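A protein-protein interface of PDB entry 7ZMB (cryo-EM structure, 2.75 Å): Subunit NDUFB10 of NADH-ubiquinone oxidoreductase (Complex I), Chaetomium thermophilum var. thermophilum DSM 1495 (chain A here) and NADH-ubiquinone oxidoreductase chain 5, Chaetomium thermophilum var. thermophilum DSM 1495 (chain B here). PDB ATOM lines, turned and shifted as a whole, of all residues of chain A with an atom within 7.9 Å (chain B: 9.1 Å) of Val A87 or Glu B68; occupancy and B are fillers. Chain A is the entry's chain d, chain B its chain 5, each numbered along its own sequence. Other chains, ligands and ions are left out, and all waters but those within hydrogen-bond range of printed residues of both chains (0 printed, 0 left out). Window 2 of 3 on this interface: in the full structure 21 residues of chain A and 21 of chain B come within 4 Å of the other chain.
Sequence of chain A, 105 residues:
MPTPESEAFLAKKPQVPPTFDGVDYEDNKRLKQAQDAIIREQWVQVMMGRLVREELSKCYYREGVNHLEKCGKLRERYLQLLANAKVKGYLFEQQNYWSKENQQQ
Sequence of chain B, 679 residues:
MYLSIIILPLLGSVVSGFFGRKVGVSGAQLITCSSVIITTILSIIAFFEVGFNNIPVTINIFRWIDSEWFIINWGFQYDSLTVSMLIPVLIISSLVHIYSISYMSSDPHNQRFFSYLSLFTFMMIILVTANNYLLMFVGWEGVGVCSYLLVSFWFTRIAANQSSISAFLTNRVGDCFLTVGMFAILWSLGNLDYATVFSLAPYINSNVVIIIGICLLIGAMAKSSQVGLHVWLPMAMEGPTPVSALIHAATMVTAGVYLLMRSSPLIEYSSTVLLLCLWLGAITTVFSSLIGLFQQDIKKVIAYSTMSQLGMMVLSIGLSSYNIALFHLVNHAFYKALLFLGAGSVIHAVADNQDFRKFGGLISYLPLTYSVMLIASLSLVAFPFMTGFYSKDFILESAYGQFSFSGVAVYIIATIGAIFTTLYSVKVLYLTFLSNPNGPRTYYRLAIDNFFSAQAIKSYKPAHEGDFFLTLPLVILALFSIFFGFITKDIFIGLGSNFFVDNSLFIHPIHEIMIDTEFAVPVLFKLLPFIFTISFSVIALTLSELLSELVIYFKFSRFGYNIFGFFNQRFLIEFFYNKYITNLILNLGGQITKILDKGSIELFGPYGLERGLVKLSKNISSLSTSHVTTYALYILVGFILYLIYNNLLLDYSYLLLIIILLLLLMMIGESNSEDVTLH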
ATOM      1  N   ILE A  38      17.587  -4.218  -2.101  1.00  0.00           N
ATOM      2  CA  ILE A  38      16.230  -4.170  -1.483  1.00  0.00           C
ATOM      3  C   ILE A  38      16.466  -3.691  -0.050  1.00  0.00           C
ATOM      4  O   ILE A  38      15.644  -2.914   0.460  1.00  0.00           O
ATOM      5  CB  ILE A  38      15.557  -5.558  -1.517  1.00  0.00           C
ATOM      6  CG1 ILE A  38      15.135  -5.943  -2.936  1.00  0.00           C
ATOM      7  CG2 ILE A  38      14.389  -5.640  -0.549  1.00  0.00           C
ATOM      8  CD1 ILE A  38      14.272  -7.175  -3.008  1.00  0.00           C
ATOM      9  N   ILE A  39      17.601  -4.078   0.536  1.00  0.00           N
ATOM     10  CA  ILE A  39      17.938  -3.593   1.867  1.00  0.00           C
ATOM     11  C   ILE A  39      18.221  -2.096   1.849  1.00  0.00           C
ATOM     12  O   ILE A  39      17.922  -1.391   2.820  1.00  0.00           O
ATOM     13  CB  ILE A  39      19.124  -4.394   2.437  1.00  0.00           C
ATOM     14  CG1 ILE A  39      18.715  -5.846   2.687  1.00  0.00           C
ATOM     15  CG2 ILE A  39      19.614  -3.790   3.726  1.00  0.00           C
ATOM     16  CD1 ILE A  39      17.414  -6.001   3.396  1.00  0.00           C
ATOM     17  N   ARG A  40      18.865  -1.607   0.790  1.00  0.00           N
ATOM     18  CA  ARG A  40      19.265  -0.174   0.697  1.00  0.00           C
ATOM     19  C   ARG A  40      18.034   0.736   0.694  1.00  0.00           C
ATOM     20  O   ARG A  40      18.102   1.803   1.318  1.00  0.00           O
ATOM     21  CB  ARG A  40      20.089   0.065  -0.569  1.00  0.00           C
ATOM     22  CG  ARG A  40      21.452  -0.608  -0.563  1.00  0.00           C
ATOM     23  CD  ARG A  40      22.472   0.111   0.289  1.00  0.00           C
ATOM     24  NE  ARG A  40      23.636  -0.733   0.484  1.00  0.00           N
ATOM     25  CZ  ARG A  40      24.763  -0.337   1.052  1.00  0.00           C
ATOM     26  NH1 ARG A  40      24.890   0.906   1.478  1.00  0.00           N
ATOM     27  NH2 ARG A  40      25.762  -1.188   1.188  1.00  0.00           N
ATOM     28  N   GLU A  41      16.952   0.324   0.031  1.00  0.00           N
ATOM     29  CA  GLU A  41      15.750   1.187  -0.119  1.00  0.00           C
ATOM     30  C   GLU A  41      14.969   1.249   1.192  1.00  0.00           C
ATOM     31  O   GLU A  41      14.577   2.357   1.589  1.00  0.00           O
ATOM     32  CB  GLU A  41      14.848   0.625  -1.213  1.00  0.00           C
ATOM     33  CG  GLU A  41      13.636   1.492  -1.506  1.00  0.00           C
ATOM     34  CD  GLU A  41      13.951   2.883  -2.031  1.00  0.00           C
ATOM     35  OE1 GLU A  41      14.945   3.025  -2.771  1.00  0.00           O
ATOM     36  OE2 GLU A  41      13.204   3.821  -1.692  1.00  0.00           O
ATOM     37  N   GLN A  42      14.752   0.097   1.820  1.00  0.00           N
ATOM     38  CA  GLN A  42      13.989   0.029   3.085  1.00  0.00           C
ATOM     39  C   GLN A  42      14.708   0.894   4.111  1.00  0.00           C
ATOM     40  O   GLN A  42      14.019   1.562   4.894  1.00  0.00           O
ATOM     41  CB  GLN A  42      13.902  -1.417   3.576  1.00  0.00           C
ATOM     42  CG  GLN A  42      13.055  -2.329   2.709  1.00  0.00           C
ATOM     43  CD  GLN A  42      13.058  -3.719   3.293  1.00  0.00           C
ATOM     44  OE1 GLN A  42      13.900  -4.055   4.119  1.00  0.00           O
ATOM     45  NE2 GLN A  42      12.110  -4.537   2.866  1.00  0.00           N
ATOM     46  N   TRP A  43      16.040   0.911   4.061  1.00  0.00           N
ATOM     47  CA  TRP A  43      16.803   1.671   5.078  1.00  0.00           C
ATOM     48  C   TRP A  43      16.709   3.163   4.742  1.00  0.00           C
ATOM     49  O   TRP A  43      16.484   3.932   5.679  1.00  0.00           O
ATOM     50  CB  TRP A  43      18.258   1.185   5.148  1.00  0.00           C
ATOM     51  CG  TRP A  43      18.520   0.220   6.263  1.00  0.00           C
ATOM     52  CD1 TRP A  43      18.748  -1.120   6.162  1.00  0.00           C
ATOM     53  CD2 TRP A  43      18.574   0.528   7.667  1.00  0.00           C
ATOM     54  NE1 TRP A  43      18.944  -1.666   7.400  1.00  0.00           N
ATOM     55  CE2 TRP A  43      18.842  -0.680   8.345  1.00  0.00           C
ATOM     56  CE3 TRP A  43      18.423   1.700   8.415  1.00  0.00           C
ATOM     57  CZ2 TRP A  43      18.955  -0.745   9.731  1.00  0.00           C
ATOM     58  CZ3 TRP A  43      18.538   1.635   9.784  1.00  0.00           C
ATOM     59  CH2 TRP A  43      18.801   0.428  10.431  1.00  0.00           C
ATOM     60  N   VAL A  44      16.814   3.553   3.468  1.00  0.00           N
ATOM     61  CA  VAL A  44      16.642   4.960   3.117  1.00  0.00           C
ATOM     62  C   VAL A  44      15.258   5.440   3.520  1.00  0.00           C
ATOM     63  O   VAL A  44      15.100   6.535   4.070  1.00  0.00           O
ATOM     64  CB  VAL A  44      16.898   5.184   1.615  1.00  0.00           C
ATOM     65  CG1 VAL A  44      16.265   6.491   1.160  1.00  0.00           C
ATOM     66  CG2 VAL A  44      18.383   5.200   1.340  1.00  0.00           C
ATOM     67  N   GLN A  45      14.239   4.620   3.268  1.00  0.00           N
ATOM     68  CA  GLN A  45      12.875   5.007   3.600  1.00  0.00           C
ATOM     69  C   GLN A  45      12.713   5.246   5.091  1.00  0.00           C
ATOM     70  O   GLN A  45      12.043   6.200   5.501  1.00  0.00           O
ATOM     71  CB  GLN A  45      11.900   3.937   3.117  1.00  0.00           C
ATOM     72  CG  GLN A  45      11.574   4.039   1.654  1.00  0.00           C
ATOM     73  CD  GLN A  45      11.347   5.470   1.221  1.00  0.00           C
ATOM     74  OE1 GLN A  45      12.182   6.065   0.541  1.00  0.00           O
ATOM     75  NE2 GLN A  45      10.215   6.034   1.618  1.00  0.00           N
ATOM     76  N   VAL A  46      13.312   4.389   5.920  1.00  0.00           N
ATOM     77  CA  VAL A  46      13.252   4.578   7.366  1.00  0.00           C
ATOM     78  C   VAL A  46      13.963   5.861   7.764  1.00  0.00           C
ATOM     79  O   VAL A  46      13.494   6.601   8.636  1.00  0.00           O
ATOM     80  CB  VAL A  46      13.838   3.357   8.097  1.00  0.00           C
ATOM     81  CG1 VAL A  46      13.875   3.597   9.596  1.00  0.00           C
ATOM     82  CG2 VAL A  46      13.032   2.121   7.796  1.00  0.00           C
ATOM     83  N   MET A  47      15.106   6.147   7.138  1.00  0.00           N
ATOM     84  CA  MET A  47      15.847   7.344   7.513  1.00  0.00           C
ATOM     85  C   MET A  47      15.180   8.623   7.041  1.00  0.00           C
ATOM     86  O   MET A  47      15.521   9.694   7.545  1.00  0.00           O
ATOM     87  CB  MET A  47      17.275   7.289   6.990  1.00  0.00           C
ATOM     88  CG  MET A  47      17.964   5.998   7.289  1.00  0.00           C
ATOM     89  SD  MET A  47      18.095   5.596   9.029  1.00  0.00           S
ATOM     90  CE  MET A  47      19.255   6.828   9.554  1.00  0.00           C
ATOM     91  N   GLY A  49      12.109   9.101   7.721  1.00  0.00           N
ATOM     92  CA  GLY A  49      11.364   9.332   8.971  1.00  0.00           C
ATOM     93  C   GLY A  49      12.249  10.061   9.966  1.00  0.00           C
ATOM     94  O   GLY A  49      11.745  10.971  10.641  1.00  0.00           O
ATOM     95  N   ARG A  50      13.530   9.697  10.040  1.00  0.00           N
ATOM     96  CA  ARG A  50      14.445  10.283  11.007  1.00  0.00           C
ATOM     97  C   ARG A  50      14.781  11.735  10.696  1.00  0.00           C
ATOM     98  O   ARG A  50      15.236  12.456  11.588  1.00  0.00           O
ATOM     99  CB  ARG A  50      15.725   9.456  11.088  1.00  0.00           C
ATOM    100  CG  ARG A  50      15.625   8.332  12.093  1.00  0.00           C
ATOM    101  CD  ARG A  50      16.780   7.380  11.982  1.00  0.00           C
ATOM    102  NE  ARG A  50      18.036   8.033  12.321  1.00  0.00           N
ATOM    103  CZ  ARG A  50      19.038   7.430  12.946  1.00  0.00           C
ATOM    104  NH1 ARG A  50      20.150   8.098  13.218  1.00  0.00           N
ATOM    105  NH2 ARG A  50      18.926   6.162  13.302  1.00  0.00           N
ATOM    106  N   ARG A  53      11.376  13.934  11.482  1.00  0.00           N
ATOM    107  CA  ARG A  53      11.105  14.047  12.934  1.00  0.00           C
ATOM    108  C   ARG A  53      12.027  15.147  13.416  1.00  0.00           C
ATOM    109  O   ARG A  53      11.580  15.980  14.206  1.00  0.00           O
ATOM    110  CB  ARG A  53      11.385  12.728  13.649  1.00  0.00           C
ATOM    111  CG  ARG A  53      10.140  12.043  14.188  1.00  0.00           C
ATOM    112  CD  ARG A  53      10.420  10.929  15.180  1.00  0.00           C
ATOM    113  NE  ARG A  53      11.215   9.822  14.668  1.00  0.00           N
ATOM    114  CZ  ARG A  53      12.502   9.638  14.929  1.00  0.00           C
ATOM    115  NH1 ARG A  53      13.137   8.593  14.425  1.00  0.00           N
ATOM    116  NH2 ARG A  53      13.150  10.496  15.697  1.00  0.00           N
ATOM    117  N   ASN A  84       4.771   3.149   6.840  1.00  0.00           N
ATOM    118  CA  ASN A  84       5.330   2.345   5.762  1.00  0.00           C
ATOM    119  C   ASN A  84       6.787   1.980   5.990  1.00  0.00           C
ATOM    120  O   ASN A  84       7.148   0.802   5.899  1.00  0.00           O
ATOM    121  CB  ASN A  84       5.194   3.098   4.432  1.00  0.00           C
ATOM    122  CG  ASN A  84       3.758   3.332   4.044  1.00  0.00           C
ATOM    123  OD1 ASN A  84       3.021   2.387   3.776  1.00  0.00           O
ATOM    124  ND2 ASN A  84       3.351   4.595   3.996  1.00  0.00           N
ATOM    125  N   ALA A  85       7.629   2.954   6.302  1.00  0.00           N
ATOM    126  CA  ALA A  85       9.077   2.763   6.288  1.00  0.00           C
ATOM    127  C   ALA A  85       9.482   1.849   7.431  1.00  0.00           C
ATOM    128  O   ALA A  85       9.635   2.287   8.571  1.00  0.00           O
ATOM    129  CB  ALA A  85       9.785   4.107   6.383  1.00  0.00           C
ATOM    130  N   LYS A  86       9.676   0.571   7.126  1.00  0.00           N
ATOM    131  CA  LYS A  86      10.155  -0.387   8.110  1.00  0.00           C
ATOM    132  C   LYS A  86      11.104  -1.349   7.423  1.00  0.00           C
ATOM    133  O   LYS A  86      10.770  -1.901   6.373  1.00  0.00           O
ATOM    134  CB  LYS A  86       9.001  -1.150   8.759  1.00  0.00           C
ATOM    135  CG  LYS A  86       9.414  -1.970   9.950  1.00  0.00           C
ATOM    136  CD  LYS A  86       8.298  -2.896  10.396  1.00  0.00           C
ATOM    137  CE  LYS A  86       8.246  -3.023  11.911  1.00  0.00           C
ATOM    138  NZ  LYS A  86       7.717  -1.790  12.559  1.00  0.00           N
ATOM    139  N   VAL A  87      12.283  -1.554   8.009  1.00  0.00           N
ATOM    140  CA  VAL A  87      13.225  -2.565   7.461  1.00  0.00           C
ATOM    141  C   VAL A  87      12.582  -3.943   7.655  1.00  0.00           C
ATOM    142  O   VAL A  87      12.362  -4.324   8.820  1.00  0.00           O
ATOM    143  CB  VAL A  87      14.608  -2.445   8.126  1.00  0.00           C
ATOM    144  CG1 VAL A  87      15.472  -3.664   7.865  1.00  0.00           C
ATOM    145  CG2 VAL A  87      15.321  -1.173   7.700  1.00  0.00           C
ATOM    146  N   LYS A  88      12.249  -4.638   6.566  1.00  0.00           N
ATOM    147  CA  LYS A  88      11.554  -5.948   6.697  1.00  0.00           C
ATOM    148  C   LYS A  88      12.421  -7.060   6.106  1.00  0.00           C
ATOM    149  O   LYS A  88      12.019  -8.225   6.200  1.00  0.00           O
ATOM    150  CB  LYS A  88      10.137  -5.869   6.129  1.00  0.00           C
ATOM    151  CG  LYS A  88       9.112  -5.178   7.016  1.00  0.00           C
ATOM    152  CD  LYS A  88       8.977  -5.810   8.380  1.00  0.00           C
ATOM    153  CE  LYS A  88       8.431  -7.221   8.350  1.00  0.00           C
ATOM    154  NZ  LYS A  88       8.315  -7.789   9.714  1.00  0.00           N
ATOM    155  N   GLY A  89      13.577  -6.701   5.546  1.00  0.00           N
ATOM    156  CA  GLY A  89      14.497  -7.697   4.977  1.00  0.00           C
ATOM    157  C   GLY A  89      14.241  -8.032   3.522  1.00  0.00           C
ATOM    158  O   GLY A  89      13.386  -7.375   2.921  1.00  0.00           O
ATOM    159  N   TYR A  90      14.981  -9.000   2.970  1.00  0.00           N
ATOM    160  CA  TYR A  90      14.860  -9.394   1.541  1.00  0.00           C
ATOM    161  C   TYR A  90      14.411 -10.846   1.414  1.00  0.00           C
ATOM    162  O   TYR A  90      14.330 -11.322   0.285  1.00  0.00           O
ATOM    163  CB  TYR A  90      16.236  -9.311   0.884  1.00  0.00           C
ATOM    164  CG  TYR A  90      17.330 -10.141   1.512  1.00  0.00           C
ATOM    165  CD1 TYR A  90      17.407 -11.507   1.307  1.00  0.00           C
ATOM    166  CD2 TYR A  90      18.320  -9.552   2.280  1.00  0.00           C
ATOM    167  CE1 TYR A  90      18.407 -12.275   1.876  1.00  0.00           C
ATOM    168  CE2 TYR A  90      19.335 -10.303   2.849  1.00  0.00           C
ATOM    169  CZ  TYR A  90      19.381 -11.669   2.642  1.00  0.00           C
ATOM    170  OH  TYR A  90      20.372 -12.428   3.192  1.00  0.00           O
ATOM    171  N   ILE B  65      21.025   5.338  21.697  1.00  0.00           N
ATOM    172  CA  ILE B  65      20.636   4.145  20.949  1.00  0.00           C
ATOM    173  C   ILE B  65      20.252   4.587  19.542  1.00  0.00           C
ATOM    174  O   ILE B  65      19.664   5.658  19.359  1.00  0.00           O
ATOM    175  CB  ILE B  65      19.481   3.363  21.617  1.00  0.00           C
ATOM    176  CG1 ILE B  65      19.879   2.814  22.987  1.00  0.00           C
ATOM    177  CG2 ILE B  65      19.032   2.192  20.767  1.00  0.00           C
ATOM    178  CD1 ILE B  65      19.590   3.734  24.133  1.00  0.00           C
ATOM    179  N   ASP B  66      20.672   3.795  18.561  1.00  0.00           N
ATOM    180  CA  ASP B  66      20.390   4.107  17.143  1.00  0.00           C
ATOM    181  C   ASP B  66      20.044   2.765  16.500  1.00  0.00           C
ATOM    182  O   ASP B  66      20.986   2.017  16.213  1.00  0.00           O
ATOM    183  CB  ASP B  66      21.599   4.805  16.518  1.00  0.00           C
ATOM    184  CG  ASP B  66      21.405   5.277  15.090  1.00  0.00           C
ATOM    185  OD1 ASP B  66      20.787   4.540  14.304  1.00  0.00           O
ATOM    186  OD2 ASP B  66      21.885   6.380  14.776  1.00  0.00           O
ATOM    187  N   SER B  67      18.757   2.428  16.410  1.00  0.00           N
ATOM    188  CA  SER B  67      18.317   1.169  15.762  1.00  0.00           C
ATOM    189  C   SER B  67      17.096   1.464  14.890  1.00  0.00           C
ATOM    190  O   SER B  67      15.997   1.594  15.455  1.00  0.00           O
ATOM    191  CB  SER B  67      17.999   0.120  16.794  1.00  0.00           C
ATOM    192  OG  SER B  67      17.469  -1.049  16.188  1.00  0.00           O
ATOM    193  N   GLU B  68      17.285   1.552  13.571  1.00  0.00           N
ATOM    194  CA  GLU B  68      16.158   1.836  12.653  1.00  0.00           C
ATOM    195  C   GLU B  68      15.482   3.140  13.090  1.00  0.00           C
ATOM    196  O   GLU B  68      16.187   4.162  13.137  1.00  0.00           O
ATOM    197  CB  GLU B  68      15.229   0.625  12.585  1.00  0.00           C
ATOM    198  CG  GLU B  68      14.325   0.568  11.374  1.00  0.00           C
ATOM    199  CD  GLU B  68      12.998  -0.086  11.708  1.00  0.00           C
ATOM    200  OE1 GLU B  68      12.514   0.121  12.835  1.00  0.00           O
ATOM    201  OE2 GLU B  68      12.467  -0.820  10.855  1.00  0.00           O
ATOM    202  N   TRP B  69      14.186   3.097  13.411  1.00  0.00           N
ATOM    203  CA  TRP B  69      13.373   4.289  13.767  1.00  0.00           C
ATOM    204  C   TRP B  69      13.728   4.827  15.138  1.00  0.00           C
ATOM    205  O   TRP B  69      13.150   5.850  15.528  1.00  0.00           O
ATOM    206  CB  TRP B  69      11.951   3.757  13.939  1.00  0.00           C
ATOM    207  CG  TRP B  69      11.095   3.679  12.725  1.00  0.00           C
ATOM    208  CD1 TRP B  69      10.544   2.556  12.189  1.00  0.00           C
ATOM    209  CD2 TRP B  69      10.633   4.783  11.934  1.00  0.00           C
ATOM    210  NE1 TRP B  69       9.781   2.886  11.109  1.00  0.00           N
ATOM    211  CE2 TRP B  69       9.824   4.241  10.918  1.00  0.00           C
ATOM    212  CE3 TRP B  69      10.833   6.164  11.979  1.00  0.00           C
ATOM    213  CZ2 TRP B  69       9.218   5.037   9.951  1.00  0.00           C
ATOM    214  CZ3 TRP B  69      10.234   6.946  11.020  1.00  0.00           C
ATOM    215  CH2 TRP B  69       9.437   6.390  10.022  1.00  0.00           C
ATOM    216  N   PHE B  70      14.696   4.233  15.805  1.00  0.00           N
ATOM    217  CA  PHE B  70      14.880   4.489  17.230  1.00  0.00           C
ATOM    218  C   PHE B  70      16.200   5.217  17.384  1.00  0.00           C
ATOM    219  O   PHE B  70      17.266   4.601  17.313  1.00  0.00           O
ATOM    220  CB  PHE B  70      14.872   3.199  18.038  1.00  0.00           C
ATOM    221  CG  PHE B  70      13.519   2.567  18.173  1.00  0.00           C
ATOM    222  CD1 PHE B  70      12.413   3.109  17.557  1.00  0.00           C
ATOM    223  CD2 PHE B  70      13.359   1.419  18.928  1.00  0.00           C
ATOM    224  CE1 PHE B  70      11.176   2.522  17.682  1.00  0.00           C
ATOM    225  CE2 PHE B  70      12.122   0.826  19.056  1.00  0.00           C
ATOM    226  CZ  PHE B  70      11.033   1.382  18.435  1.00  0.00           C
ATOM    227  N   ILE B  71      16.137   6.525  17.587  1.00  0.00           N
ATOM    228  CA  ILE B  71      17.328   7.350  17.745  1.00  0.00           C
ATOM    229  C   ILE B  71      17.154   8.141  19.037  1.00  0.00           C
ATOM    230  O   ILE B  71      16.595   9.241  19.055  1.00  0.00           O
ATOM    231  CB  ILE B  71      17.587   8.257  16.539  1.00  0.00           C
ATOM    232  CG1 ILE B  71      18.793   9.156  16.810  1.00  0.00           C
ATOM    233  CG2 ILE B  71      16.323   8.998  16.114  1.00  0.00           C
ATOM    234  CD1 ILE B  71      20.072   8.394  17.023  1.00  0.00           C
ATOM    235  N   ILE B  72      17.633   7.574  20.131  1.00  0.00           N
ATOM    236  CA  ILE B  72      17.581   8.211  21.434  1.00  0.00           C
ATOM    237  C   ILE B  72      18.918   8.883  21.667  1.00  0.00           C
ATOM    238  O   ILE B  72      19.968   8.242  21.567  1.00  0.00           O
ATOM    239  CB  ILE B  72      17.259   7.195  22.535  1.00  0.00           C
ATOM    240  CG1 ILE B  72      15.921   6.553  22.215  1.00  0.00           C
ATOM    241  CG2 ILE B  72      17.247   7.855  23.897  1.00  0.00           C
ATOM    242  CD1 ILE B  72      14.817   7.551  22.167  1.00  0.00           C
ATOM    243  N   LEU B 186       7.183   3.540  21.977  1.00  0.00           N
ATOM    244  CA  LEU B 186       8.038   3.181  20.848  1.00  0.00           C
ATOM    245  C   LEU B 186       7.265   2.409  19.793  1.00  0.00           C
ATOM    246  O   LEU B 186       7.531   2.551  18.597  1.00  0.00           O
ATOM    247  CB  LEU B 186       9.230   2.354  21.327  1.00  0.00           C
ATOM    248  CG  LEU B 186      10.429   3.123  21.859  1.00  0.00           C
ATOM    249  CD1 LEU B 186      11.538   2.162  22.235  1.00  0.00           C
ATOM    250  CD2 LEU B 186      10.908   4.119  20.830  1.00  0.00           C
ATOM    251  N   GLY B 190       7.089   5.145  17.018  1.00  0.00           N
ATOM    252  CA  GLY B 190       8.398   4.924  16.381  1.00  0.00           C
ATOM    253  C   GLY B 190       9.517   5.637  17.103  1.00  0.00           C
ATOM    254  O   GLY B 190      10.667   5.469  16.695  1.00  0.00           O
ATOM    255  N   ASN B 191       9.186   6.451  18.096  1.00  0.00           N
ATOM    256  CA  ASN B 191      10.231   7.110  18.924  1.00  0.00           C
ATOM    257  C   ASN B 191       9.612   7.535  20.249  1.00  0.00           C
ATOM    258  O   ASN B 191       8.434   7.245  20.466  1.00  0.00           O
ATOM    259  CB  ASN B 191      10.945   8.270  18.222  1.00  0.00           C
ATOM    260  CG  ASN B 191      12.435   8.295  18.484  1.00  0.00           C
ATOM    261  OD1 ASN B 191      13.126   7.303  18.267  1.00  0.00           O
ATOM    262  ND2 ASN B 191      12.940   9.426  18.943  1.00  0.00           N
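Hydrophobic or aromatic side chains of chain A within 4 Å of the printed part of chain B: Trp A43, Val A46, Ala A85 and Val A87.
Of the 11 printed residues of chain B, 5 touch a printed residue of chain A.
Printed residues of chain B that touch a printed residue of chain A: Asp B66, Glu B68, Trp B69, Ile B71 and Asn B191.
Among the printed residues, 13 pairs touch across the chains.
Val A87 touches just one residue of chain B: Glu B68 (2.9 Å).
No residue of chain A comes within 4 Å of Ser B67.
Printed residues of chain A within 4 Å of Asn B191: Arg A53 (3.4 Å).
Of the printed residues of chain A, Asp B66 touches Arg A50.
Leu B186 touches none of the printed residues of chain A.
Gln A45 touches none of the printed residues of chain B.
The nearest printed residue of chain B that does not touch Trp A43 is Ser B67 (4.9 Å).
Glu B68 touches Trp A43 (N to CH2, 3.7 Å).
Val A46 touches Glu B68.
Trp B69 touches Val A46 (N to CG1, 3.9 Å).
CA of Gly A49 touches CZ3 of Trp B69 (3.3 Å).
Ile B71 touches Arg A50.
Ile B71 touches Arg A53.
OE2 of Glu B68 touches CG of Lys A86, 3.4 Å away.
The side-chain amide oxygen (OD1) of Asn B191 lies close to the backbone carbonyl oxygen (O) of Trp B69 (3.1 Å).
The side-chain amide oxygen (OD1) of Asn B191 is in hydrogen-bond range of the backbone NH (N) of Ile B71, 3.2 Å away.
The guanidinium group (NH2) of Arg A50 lies within salt-bridge range of the side-chain carboxylate (OD1) of Asp B66.
O of Glu B68 is in hydrogen-bond range of NH2 of Arg A50 (3.4 Å).
The backbone carbonyl oxygen (O) of Trp B69 sits at hydrogen-bond distance from the guanidinium group (NH1) of Arg A53, at 3.0 Å.
The guanidinium group (NH2) of Arg A53 lies close to the side-chain amide nitrogen (ND2) of Asn B191 (3.4 Å).
NE1 of Trp B69 lies within hydrogen-bond range of O of Ala A85 (2.6 Å).
The side-chain carboxylate of Glu B68 sits at hydrogen-bond distance from the backbone NH of Val A87 (2.9 Å).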
